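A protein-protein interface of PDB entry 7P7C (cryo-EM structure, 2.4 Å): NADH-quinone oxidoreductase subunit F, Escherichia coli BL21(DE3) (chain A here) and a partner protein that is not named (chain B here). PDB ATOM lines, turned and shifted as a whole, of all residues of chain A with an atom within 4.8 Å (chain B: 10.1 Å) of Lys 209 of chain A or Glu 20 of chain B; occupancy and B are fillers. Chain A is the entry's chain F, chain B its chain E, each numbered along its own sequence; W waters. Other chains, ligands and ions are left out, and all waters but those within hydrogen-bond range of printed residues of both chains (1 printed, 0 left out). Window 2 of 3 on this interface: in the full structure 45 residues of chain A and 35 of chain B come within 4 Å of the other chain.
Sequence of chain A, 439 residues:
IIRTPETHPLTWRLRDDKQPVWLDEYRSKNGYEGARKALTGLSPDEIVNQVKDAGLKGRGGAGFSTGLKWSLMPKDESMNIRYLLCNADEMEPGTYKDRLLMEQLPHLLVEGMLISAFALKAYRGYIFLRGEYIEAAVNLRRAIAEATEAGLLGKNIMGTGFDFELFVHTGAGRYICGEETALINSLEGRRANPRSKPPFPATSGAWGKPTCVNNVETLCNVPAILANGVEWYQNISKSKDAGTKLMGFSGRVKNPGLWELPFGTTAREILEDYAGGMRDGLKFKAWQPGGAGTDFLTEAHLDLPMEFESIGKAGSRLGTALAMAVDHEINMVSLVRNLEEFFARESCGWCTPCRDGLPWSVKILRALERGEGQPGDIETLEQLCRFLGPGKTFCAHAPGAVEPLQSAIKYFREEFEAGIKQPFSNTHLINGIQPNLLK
O of Pro 210 of chain A lies within hydrogen-bond range of N of Tyr 83 of chain A (3.0 Å).
The backbone carbonyl oxygen (O) of Trp 207 of chain A lies within hydrogen-bond range of the side-chain amino group (NZ) of Lys 209 of chain A (3.0 Å).
The side-chain hydroxyl (OG1) of Thr 211 of chain A lies within hydrogen-bond range of the backbone carbonyl oxygen (O) of Lys 209 of chain A, 3.0 Å away.
O of His 14 of chain B lies within hydrogen-bond range of NE2 of His 18 of chain B (3.0 Å).
The side-chain carboxylate (OD1) of Asp 21 of chain B is in hydrogen-bond range of the backbone NH (N) of Arg 23 of chain B, 2.9 Å away.
NH1 of Arg 124 of chain A touches O of His 18 of chain B, at 3.7 Å.
Arg 124 of chain A touches Tyr 19 of chain B (NH1 to C, 3.9 Å).
Arg 124 of chain A touches Glu 20 of chain B.
CD1 of Tyr 19 of chain B touches CH2 of Trp 207 of chain A (3.9 Å).
CD of Glu 20 of chain B touches CB of Trp 207 of chain A, at 3.5 Å.
Trp 207 of chain A touches Asp 21 of chain B.
Trp 207 of chain A touches Ala 24 of chain B.
Water W1 lies within hydrogen-bond range of the side-chain hydroxyl of Tyr 83 of chain A (2.8 Å), the guanidinium group of Arg 124 of chain A (3.2 Å) and the backbone NH of Glu 20 of chain B (3.3 Å).
OE1 of Glu 20 of chain B lies within salt-bridge range of NZ of Lys 209 of chain A (3.5 Å).
The side-chain hydroxyl (OH) of Tyr 83 of chain A sits close to the side-chain carboxylate (OE2) of Glu 20 of chain B (2.4 Å).
Of the printed residues of chain B, Tyr 83 of chain A touches Glu 20.
No residue of chain B comes within 4 Å of Gly 205 of chain A.
No residue of chain B comes within 4 Å of Ala 206 of chain A.
Of chain B, only Tyr 19 (3.9 Å), Glu 20 (3.5 Å), Asp 21 (3.6 Å) and Ala 24 (3.8 Å) come within 4 Å of Trp 207 of chain A.
Lys 209 of chain A touches one residue of chain B.
No residue of chain B comes within 4 Å of Pro 210 of chain A.
No residue of chain B comes within 4 Å of Thr 211 of chain A.
His 14 of chain B touches none of the printed residues of chain A.
Of chain A, only Tyr 83, Arg 124, Trp 207 and Lys 209 come within 4 Å of Glu 20 of chain B.
Printed residues of chain A within 4 Å of Asp 21 of chain B: Trp 207.
Of the printed residues of chain A, Ala 24 of chain B touches Trp 207.
The nearest residue of chain B that does not touch Lys 209 of chain A is Asp 21 of chain B (8.4 Å).
The nearest residue of chain A that does not touch Glu 20 of chain B is Ile 81 of chain A (4.2 Å).
Hydrophobic or aromatic side chains of chain B within 4 Å of the printed part of chain A: Tyr 19 and Ala 24.
Of the 13 printed residues of chain A, 4 touch a printed residue of chain B.
Among the printed residues, 9 pairs touch across the chains.
Among the printed residues, Asp or Glu carboxylates within 4 Å of a Lys or Arg side-chain nitrogen of the other chain: Lys 209 of chain A with Glu 20 of chain B (3.5 Å).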
ATOM      1  N   ILE A  81      -2.600   7.415  21.323  1.00  0.00           N
ATOM      2  CA  ILE A  81      -2.597   6.040  21.805  1.00  0.00           C
ATOM      3  C   ILE A  81      -2.375   5.145  20.594  1.00  0.00           C
ATOM      4  O   ILE A  81      -3.240   5.056  19.715  1.00  0.00           O
ATOM      5  CB  ILE A  81      -3.905   5.696  22.531  1.00  0.00           C
ATOM      6  CG1 ILE A  81      -3.994   6.461  23.852  1.00  0.00           C
ATOM      7  CG2 ILE A  81      -4.023   4.204  22.770  1.00  0.00           C
ATOM      8  CD1 ILE A  81      -2.896   6.119  24.828  1.00  0.00           C
ATOM      9  N   TYR A  83      -0.371   1.422  18.849  1.00  0.00           N
ATOM     10  CA  TYR A  83       0.010   0.045  19.124  1.00  0.00           C
ATOM     11  C   TYR A  83       0.890  -0.523  18.022  1.00  0.00           C
ATOM     12  O   TYR A  83       0.630  -0.333  16.827  1.00  0.00           O
ATOM     13  CB  TYR A  83      -1.225  -0.837  19.294  1.00  0.00           C
ATOM     14  CG  TYR A  83      -2.045  -0.475  20.499  1.00  0.00           C
ATOM     15  CD1 TYR A  83      -1.599  -0.770  21.775  1.00  0.00           C
ATOM     16  CD2 TYR A  83      -3.261   0.177  20.364  1.00  0.00           C
ATOM     17  CE1 TYR A  83      -2.340  -0.436  22.881  1.00  0.00           C
ATOM     18  CE2 TYR A  83      -4.011   0.517  21.465  1.00  0.00           C
ATOM     19  CZ  TYR A  83      -3.545   0.208  22.721  1.00  0.00           C
ATOM     20  OH  TYR A  83      -4.289   0.543  23.824  1.00  0.00           O
ATOM     21  N   ARG A 124       2.383   1.356  23.091  1.00  0.00           N
ATOM     22  CA  ARG A 124       2.393  -0.022  23.567  1.00  0.00           C
ATOM     23  C   ARG A 124       2.748  -0.994  22.454  1.00  0.00           C
ATOM     24  O   ARG A 124       2.487  -0.746  21.273  1.00  0.00           O
ATOM     25  CB  ARG A 124       1.055  -0.416  24.193  1.00  0.00           C
ATOM     26  CG  ARG A 124       1.080  -0.400  25.709  1.00  0.00           C
ATOM     27  CD  ARG A 124      -0.235  -0.857  26.303  1.00  0.00           C
ATOM     28  NE  ARG A 124      -0.231  -0.752  27.756  1.00  0.00           N
ATOM     29  CZ  ARG A 124      -1.316  -0.789  28.516  1.00  0.00           C
ATOM     30  NH1 ARG A 124      -2.523  -0.926  27.991  1.00  0.00           N
ATOM     31  NH2 ARG A 124      -1.188  -0.687  29.834  1.00  0.00           N
ATOM     32  N   PRO A 201      -5.650  -1.144   9.531  1.00  0.00           N
ATOM     33  CA  PRO A 201      -5.276  -1.020  10.950  1.00  0.00           C
ATOM     34  C   PRO A 201      -4.476   0.227  11.286  1.00  0.00           C
ATOM     35  O   PRO A 201      -4.457   0.626  12.455  1.00  0.00           O
ATOM     36  CB  PRO A 201      -4.450  -2.286  11.201  1.00  0.00           C
ATOM     37  CG  PRO A 201      -4.980  -3.263  10.236  1.00  0.00           C
ATOM     38  CD  PRO A 201      -5.340  -2.487   9.008  1.00  0.00           C
ATOM     39  N   THR A 203      -5.248   3.207  10.533  1.00  0.00           N
ATOM     40  CA  THR A 203      -6.210   4.234  10.912  1.00  0.00           C
ATOM     41  C   THR A 203      -7.019   3.827  12.139  1.00  0.00           C
ATOM     42  O   THR A 203      -7.135   4.599  13.095  1.00  0.00           O
ATOM     43  CB  THR A 203      -7.138   4.534   9.732  1.00  0.00           C
ATOM     44  OG1 THR A 203      -6.374   5.097   8.660  1.00  0.00           O
ATOM     45  CG2 THR A 203      -8.222   5.510  10.134  1.00  0.00           C
ATOM     46  N   SER A 204      -7.574   2.616  12.134  1.00  0.00           N
ATOM     47  CA  SER A 204      -8.340   2.101  13.269  1.00  0.00           C
ATOM     48  C   SER A 204      -8.070   0.605  13.366  1.00  0.00           C
ATOM     49  O   SER A 204      -8.696  -0.193  12.663  1.00  0.00           O
ATOM     50  CB  SER A 204      -9.827   2.391  13.114  1.00  0.00           C
ATOM     51  OG  SER A 204     -10.299   1.977  11.847  1.00  0.00           O
ATOM     52  N   GLY A 205      -7.138   0.231  14.235  1.00  0.00           N
ATOM     53  CA  GLY A 205      -6.761  -1.158  14.384  1.00  0.00           C
ATOM     54  C   GLY A 205      -7.137  -1.742  15.725  1.00  0.00           C
ATOM     55  O   GLY A 205      -8.315  -2.000  15.986  1.00  0.00           O
ATOM     56  N   ALA A 206      -6.143  -1.952  16.584  1.00  0.00           N
ATOM     57  CA  ALA A 206      -6.378  -2.563  17.886  1.00  0.00           C
ATOM     58  C   ALA A 206      -7.117  -1.590  18.793  1.00  0.00           C
ATOM     59  O   ALA A 206      -6.607  -0.507  19.098  1.00  0.00           O
ATOM     60  CB  ALA A 206      -5.055  -2.990  18.512  1.00  0.00           C
ATOM     61  N   TRP A 207      -8.323  -1.986  19.213  1.00  0.00           N
ATOM     62  CA  TRP A 207      -9.227  -1.173  20.032  1.00  0.00           C
ATOM     63  C   TRP A 207      -9.538   0.172  19.378  1.00  0.00           C
ATOM     64  O   TRP A 207      -9.699   1.185  20.060  1.00  0.00           O
ATOM     65  CB  TRP A 207      -8.677  -0.975  21.449  1.00  0.00           C
ATOM     66  CG  TRP A 207      -8.418  -2.263  22.169  1.00  0.00           C
ATOM     67  CD1 TRP A 207      -9.342  -3.069  22.757  1.00  0.00           C
ATOM     68  CD2 TRP A 207      -7.149  -2.896  22.369  1.00  0.00           C
ATOM     69  NE1 TRP A 207      -8.731  -4.162  23.314  1.00  0.00           N
ATOM     70  CE2 TRP A 207      -7.384  -4.081  23.088  1.00  0.00           C
ATOM     71  CE3 TRP A 207      -5.837  -2.573  22.011  1.00  0.00           C
ATOM     72  CZ2 TRP A 207      -6.358  -4.945  23.457  1.00  0.00           C
ATOM     73  CZ3 TRP A 207      -4.821  -3.432  22.377  1.00  0.00           C
ATOM     74  CH2 TRP A 207      -5.087  -4.603  23.092  1.00  0.00           C
ATOM     75  N   GLY A 208      -9.617   0.190  18.048  1.00  0.00           N
ATOM     76  CA  GLY A 208      -9.911   1.390  17.299  1.00  0.00           C
ATOM     77  C   GLY A 208      -8.760   2.359  17.146  1.00  0.00           C
ATOM     78  O   GLY A 208      -8.907   3.359  16.434  1.00  0.00           O
ATOM     79  N   LYS A 209      -7.628   2.099  17.778  1.00  0.00           N
ATOM     80  CA  LYS A 209      -6.470   2.972  17.756  1.00  0.00           C
ATOM     81  C   LYS A 209      -5.593   2.667  16.553  1.00  0.00           C
ATOM     82  O   LYS A 209      -5.702   1.596  15.951  1.00  0.00           O
ATOM     83  CB  LYS A 209      -5.669   2.805  19.043  1.00  0.00           C
ATOM     84  CG  LYS A 209      -6.500   2.931  20.300  1.00  0.00           C
ATOM     85  CD  LYS A 209      -7.186   4.278  20.373  1.00  0.00           C
ATOM     86  CE  LYS A 209      -7.895   4.452  21.702  1.00  0.00           C
ATOM     87  NZ  LYS A 209      -8.920   3.395  21.916  1.00  0.00           N
ATOM     88  N   PRO A 210      -4.752   3.616  16.143  1.00  0.00           N
ATOM     89  CA  PRO A 210      -3.740   3.314  15.120  1.00  0.00           C
ATOM     90  C   PRO A 210      -2.799   2.200  15.561  1.00  0.00           C
ATOM     91  O   PRO A 210      -2.238   2.220  16.663  1.00  0.00           O
ATOM     92  CB  PRO A 210      -3.004   4.648  14.939  1.00  0.00           C
ATOM     93  CG  PRO A 210      -3.668   5.630  15.855  1.00  0.00           C
ATOM     94  CD  PRO A 210      -4.962   5.063  16.291  1.00  0.00           C
ATOM     95  N   THR A 211      -2.632   1.224  14.674  1.00  0.00           N
ATOM     96  CA  THR A 211      -1.956  -0.026  14.973  1.00  0.00           C
ATOM     97  C   THR A 211      -1.171  -0.466  13.749  1.00  0.00           C
ATOM     98  O   THR A 211      -1.671  -0.385  12.625  1.00  0.00           O
ATOM     99  CB  THR A 211      -2.971  -1.111  15.366  1.00  0.00           C
ATOM    100  OG1 THR A 211      -3.752  -0.657  16.476  1.00  0.00           O
ATOM    101  CG2 THR A 211      -2.280  -2.397  15.745  1.00  0.00           C
ATOM    102  N   HIS B  14      -4.283  -9.846  36.889  1.00  0.00           N
ATOM    103  CA  HIS B  14      -2.970  -9.410  36.427  1.00  0.00           C
ATOM    104  C   HIS B  14      -2.880  -9.409  34.906  1.00  0.00           C
ATOM    105  O   HIS B  14      -2.213  -8.546  34.327  1.00  0.00           O
ATOM    106  CB  HIS B  14      -1.873 -10.289  37.020  1.00  0.00           C
ATOM    107  CG  HIS B  14      -0.490  -9.799  36.720  1.00  0.00           C
ATOM    108  ND1 HIS B  14       0.040  -8.671  37.307  1.00  0.00           N
ATOM    109  CD2 HIS B  14       0.464 -10.275  35.887  1.00  0.00           C
ATOM    110  CE1 HIS B  14       1.266  -8.477  36.853  1.00  0.00           C
ATOM    111  NE2 HIS B  14       1.547  -9.436  35.990  1.00  0.00           N
ATOM    112  N   GLU B  15      -3.541 -10.364  34.247  1.00  0.00           N
ATOM    113  CA  GLU B  15      -3.658 -10.311  32.794  1.00  0.00           C
ATOM    114  C   GLU B  15      -4.515  -9.134  32.346  1.00  0.00           C
ATOM    115  O   GLU B  15      -4.243  -8.534  31.301  1.00  0.00           O
ATOM    116  CB  GLU B  15      -4.238 -11.620  32.266  1.00  0.00           C
ATOM    117  CG  GLU B  15      -3.196 -12.683  31.982  1.00  0.00           C
ATOM    118  CD  GLU B  15      -2.077 -12.175  31.098  1.00  0.00           C
ATOM    119  OE1 GLU B  15      -2.370 -11.676  29.992  1.00  0.00           O
ATOM    120  OE2 GLU B  15      -0.903 -12.272  31.512  1.00  0.00           O
ATOM    121  N   MET B  16      -5.551  -8.796  33.120  1.00  0.00           N
ATOM    122  CA  MET B  16      -6.410  -7.662  32.789  1.00  0.00           C
ATOM    123  C   MET B  16      -5.663  -6.338  32.864  1.00  0.00           C
ATOM    124  O   MET B  16      -6.053  -5.375  32.195  1.00  0.00           O
ATOM    125  CB  MET B  16      -7.616  -7.619  33.723  1.00  0.00           C
ATOM    126  CG  MET B  16      -8.715  -8.599  33.384  1.00  0.00           C
ATOM    127  SD  MET B  16      -9.797  -8.895  34.793  1.00  0.00           S
ATOM    128  CE  MET B  16     -10.747  -7.380  34.810  1.00  0.00           C
ATOM    129  N   HIS B  17      -4.609  -6.265  33.681  1.00  0.00           N
ATOM    130  CA  HIS B  17      -3.826  -5.035  33.784  1.00  0.00           C
ATOM    131  C   HIS B  17      -3.131  -4.649  32.480  1.00  0.00           C
ATOM    132  O   HIS B  17      -2.869  -3.461  32.263  1.00  0.00           O
ATOM    133  CB  HIS B  17      -2.776  -5.168  34.887  1.00  0.00           C
ATOM    134  CG  HIS B  17      -3.342  -5.135  36.270  1.00  0.00           C
ATOM    135  ND1 HIS B  17      -2.934  -6.000  37.262  1.00  0.00           N
ATOM    136  CD2 HIS B  17      -4.282  -4.338  36.831  1.00  0.00           C
ATOM    137  CE1 HIS B  17      -3.598  -5.740  38.373  1.00  0.00           C
ATOM    138  NE2 HIS B  17      -4.423  -4.735  38.138  1.00  0.00           N
ATOM    139  N   HIS B  18      -2.833  -5.609  31.608  1.00  0.00           N
ATOM    140  CA  HIS B  18      -1.994  -5.367  30.439  1.00  0.00           C
ATOM    141  C   HIS B  18      -2.753  -4.833  29.232  1.00  0.00           C
ATOM    142  O   HIS B  18      -2.132  -4.578  28.197  1.00  0.00           O
ATOM    143  CB  HIS B  18      -1.264  -6.651  30.036  1.00  0.00           C
ATOM    144  CG  HIS B  18      -0.593  -7.349  31.175  1.00  0.00           C
ATOM    145  ND1 HIS B  18       0.098  -6.674  32.158  1.00  0.00           N
ATOM    146  CD2 HIS B  18      -0.499  -8.663  31.484  1.00  0.00           C
ATOM    147  CE1 HIS B  18       0.585  -7.542  33.026  1.00  0.00           C
ATOM    148  NE2 HIS B  18       0.235  -8.757  32.641  1.00  0.00           N
ATOM    149  N   TYR B  19      -4.066  -4.660  29.326  1.00  0.00           N
ATOM    150  CA  TYR B  19      -4.871  -4.235  28.192  1.00  0.00           C
ATOM    151  C   TYR B  19      -5.769  -3.077  28.595  1.00  0.00           C
ATOM    152  O   TYR B  19      -6.061  -2.869  29.775  1.00  0.00           O
ATOM    153  CB  TYR B  19      -5.727  -5.382  27.650  1.00  0.00           C
ATOM    154  CG  TYR B  19      -4.954  -6.644  27.361  1.00  0.00           C
ATOM    155  CD1 TYR B  19      -4.225  -6.779  26.188  1.00  0.00           C
ATOM    156  CD2 TYR B  19      -4.962  -7.704  28.254  1.00  0.00           C
ATOM    157  CE1 TYR B  19      -3.524  -7.932  25.917  1.00  0.00           C
ATOM    158  CE2 TYR B  19      -4.263  -8.860  27.991  1.00  0.00           C
ATOM    159  CZ  TYR B  19      -3.547  -8.968  26.822  1.00  0.00           C
ATOM    160  OH  TYR B  19      -2.847 -10.120  26.557  1.00  0.00           O
ATOM    161  N   GLU B  20      -6.208  -2.320  27.595  1.00  0.00           N
ATOM    162  CA  GLU B  20      -7.135  -1.220  27.813  1.00  0.00           C
ATOM    163  C   GLU B  20      -8.590  -1.667  27.818  1.00  0.00           C
ATOM    164  O   GLU B  20      -9.477  -0.834  28.027  1.00  0.00           O
ATOM    165  CB  GLU B  20      -6.930  -0.136  26.754  1.00  0.00           C
ATOM    166  CG  GLU B  20      -7.070  -0.614  25.325  1.00  0.00           C
ATOM    167  CD  GLU B  20      -7.487   0.497  24.387  1.00  0.00           C
ATOM    168  OE1 GLU B  20      -8.669   0.893  24.419  1.00  0.00           O
ATOM    169  OE2 GLU B  20      -6.631   0.982  23.619  1.00  0.00           O
ATOM    170  N   ASP B  21      -8.856  -2.955  27.595  1.00  0.00           N
ATOM    171  CA  ASP B  21     -10.199  -3.502  27.625  1.00  0.00           C
ATOM    172  C   ASP B  21     -10.039  -4.875  28.268  1.00  0.00           C
ATOM    173  O   ASP B  21      -9.193  -5.668  27.818  1.00  0.00           O
ATOM    174  CB  ASP B  21     -10.810  -3.606  26.221  1.00  0.00           C
ATOM    175  CG  ASP B  21     -12.291  -3.983  26.229  1.00  0.00           C
ATOM    176  OD1 ASP B  21     -12.707  -4.915  26.947  1.00  0.00           O
ATOM    177  OD2 ASP B  21     -13.056  -3.325  25.495  1.00  0.00           O
ATOM    178  N   PRO B  22     -10.815  -5.189  29.311  1.00  0.00           N
ATOM    179  CA  PRO B  22     -10.675  -6.497  29.975  1.00  0.00           C
ATOM    180  C   PRO B  22     -11.138  -7.683  29.141  1.00  0.00           C
ATOM    181  O   PRO B  22     -10.884  -8.824  29.544  1.00  0.00           O
ATOM    182  CB  PRO B  22     -11.537  -6.344  31.234  1.00  0.00           C
ATOM    183  CG  PRO B  22     -12.498  -5.259  30.904  1.00  0.00           C
ATOM    184  CD  PRO B  22     -11.753  -4.308  30.026  1.00  0.00           C
ATOM    185  N   ARG B  23     -11.818  -7.458  28.012  1.00  0.00           N
ATOM    186  CA  ARG B  23     -12.175  -8.555  27.120  1.00  0.00           C
ATOM    187  C   ARG B  23     -10.935  -9.229  26.545  1.00  0.00           C
ATOM    188  O   ARG B  23     -10.946 -10.436  26.281  1.00  0.00           O
ATOM    189  CB  ARG B  23     -13.076  -8.036  25.997  1.00  0.00           C
ATOM    190  CG  ARG B  23     -13.486  -9.068  24.959  1.00  0.00           C
ATOM    191  CD  ARG B  23     -14.139  -8.411  23.759  1.00  0.00           C
ATOM    192  NE  ARG B  23     -15.416  -7.801  24.107  1.00  0.00           N
ATOM    193  CZ  ARG B  23     -16.556  -8.465  24.223  1.00  0.00           C
ATOM    194  NH1 ARG B  23     -16.622  -9.768  24.002  1.00  0.00           N
ATOM    195  NH2 ARG B  23     -17.657  -7.807  24.569  1.00  0.00           N
ATOM    196  N   ALA B  24      -9.842  -8.479  26.400  1.00  0.00           N
ATOM    197  CA  ALA B  24      -8.613  -8.976  25.799  1.00  0.00           C
ATOM    198  C   ALA B  24      -7.899 -10.016  26.649  1.00  0.00           C
ATOM    199  O   ALA B  24      -6.947 -10.632  26.164  1.00  0.00           O
ATOM    200  CB  ALA B  24      -7.677  -7.805  25.515  1.00  0.00           C
ATOM    201  N   ALA B  25      -8.323 -10.223  27.894  1.00  0.00           N
ATOM    202  CA  ALA B  25      -7.747 -11.238  28.762  1.00  0.00           C
ATOM    203  C   ALA B  25      -8.545 -12.536  28.763  1.00  0.00           C
ATOM    204  O   ALA B  25      -8.309 -13.388  29.624  1.00  0.00           O
ATOM    205  CB  ALA B  25      -7.624 -10.699  30.186  1.00  0.00           C
ATOM    206  N   LEU B  52     -14.465 -11.020  33.994  1.00  0.00           N
ATOM    207  CA  LEU B  52     -14.070 -10.068  32.961  1.00  0.00           C
ATOM    208  C   LEU B  52     -15.155  -9.063  32.597  1.00  0.00           C
ATOM    209  O   LEU B  52     -14.853  -8.081  31.914  1.00  0.00           O
ATOM    210  CB  LEU B  52     -13.650 -10.804  31.692  1.00  0.00           C
ATOM    211  CG  LEU B  52     -12.484 -11.776  31.808  1.00  0.00           C
ATOM    212  CD1 LEU B  52     -12.302 -12.452  30.486  1.00  0.00           C
ATOM    213  CD2 LEU B  52     -11.228 -11.051  32.206  1.00  0.00           C
HETATM  214  O   HOH W   1      -3.932  -1.860  25.306  1.00  0.00           O
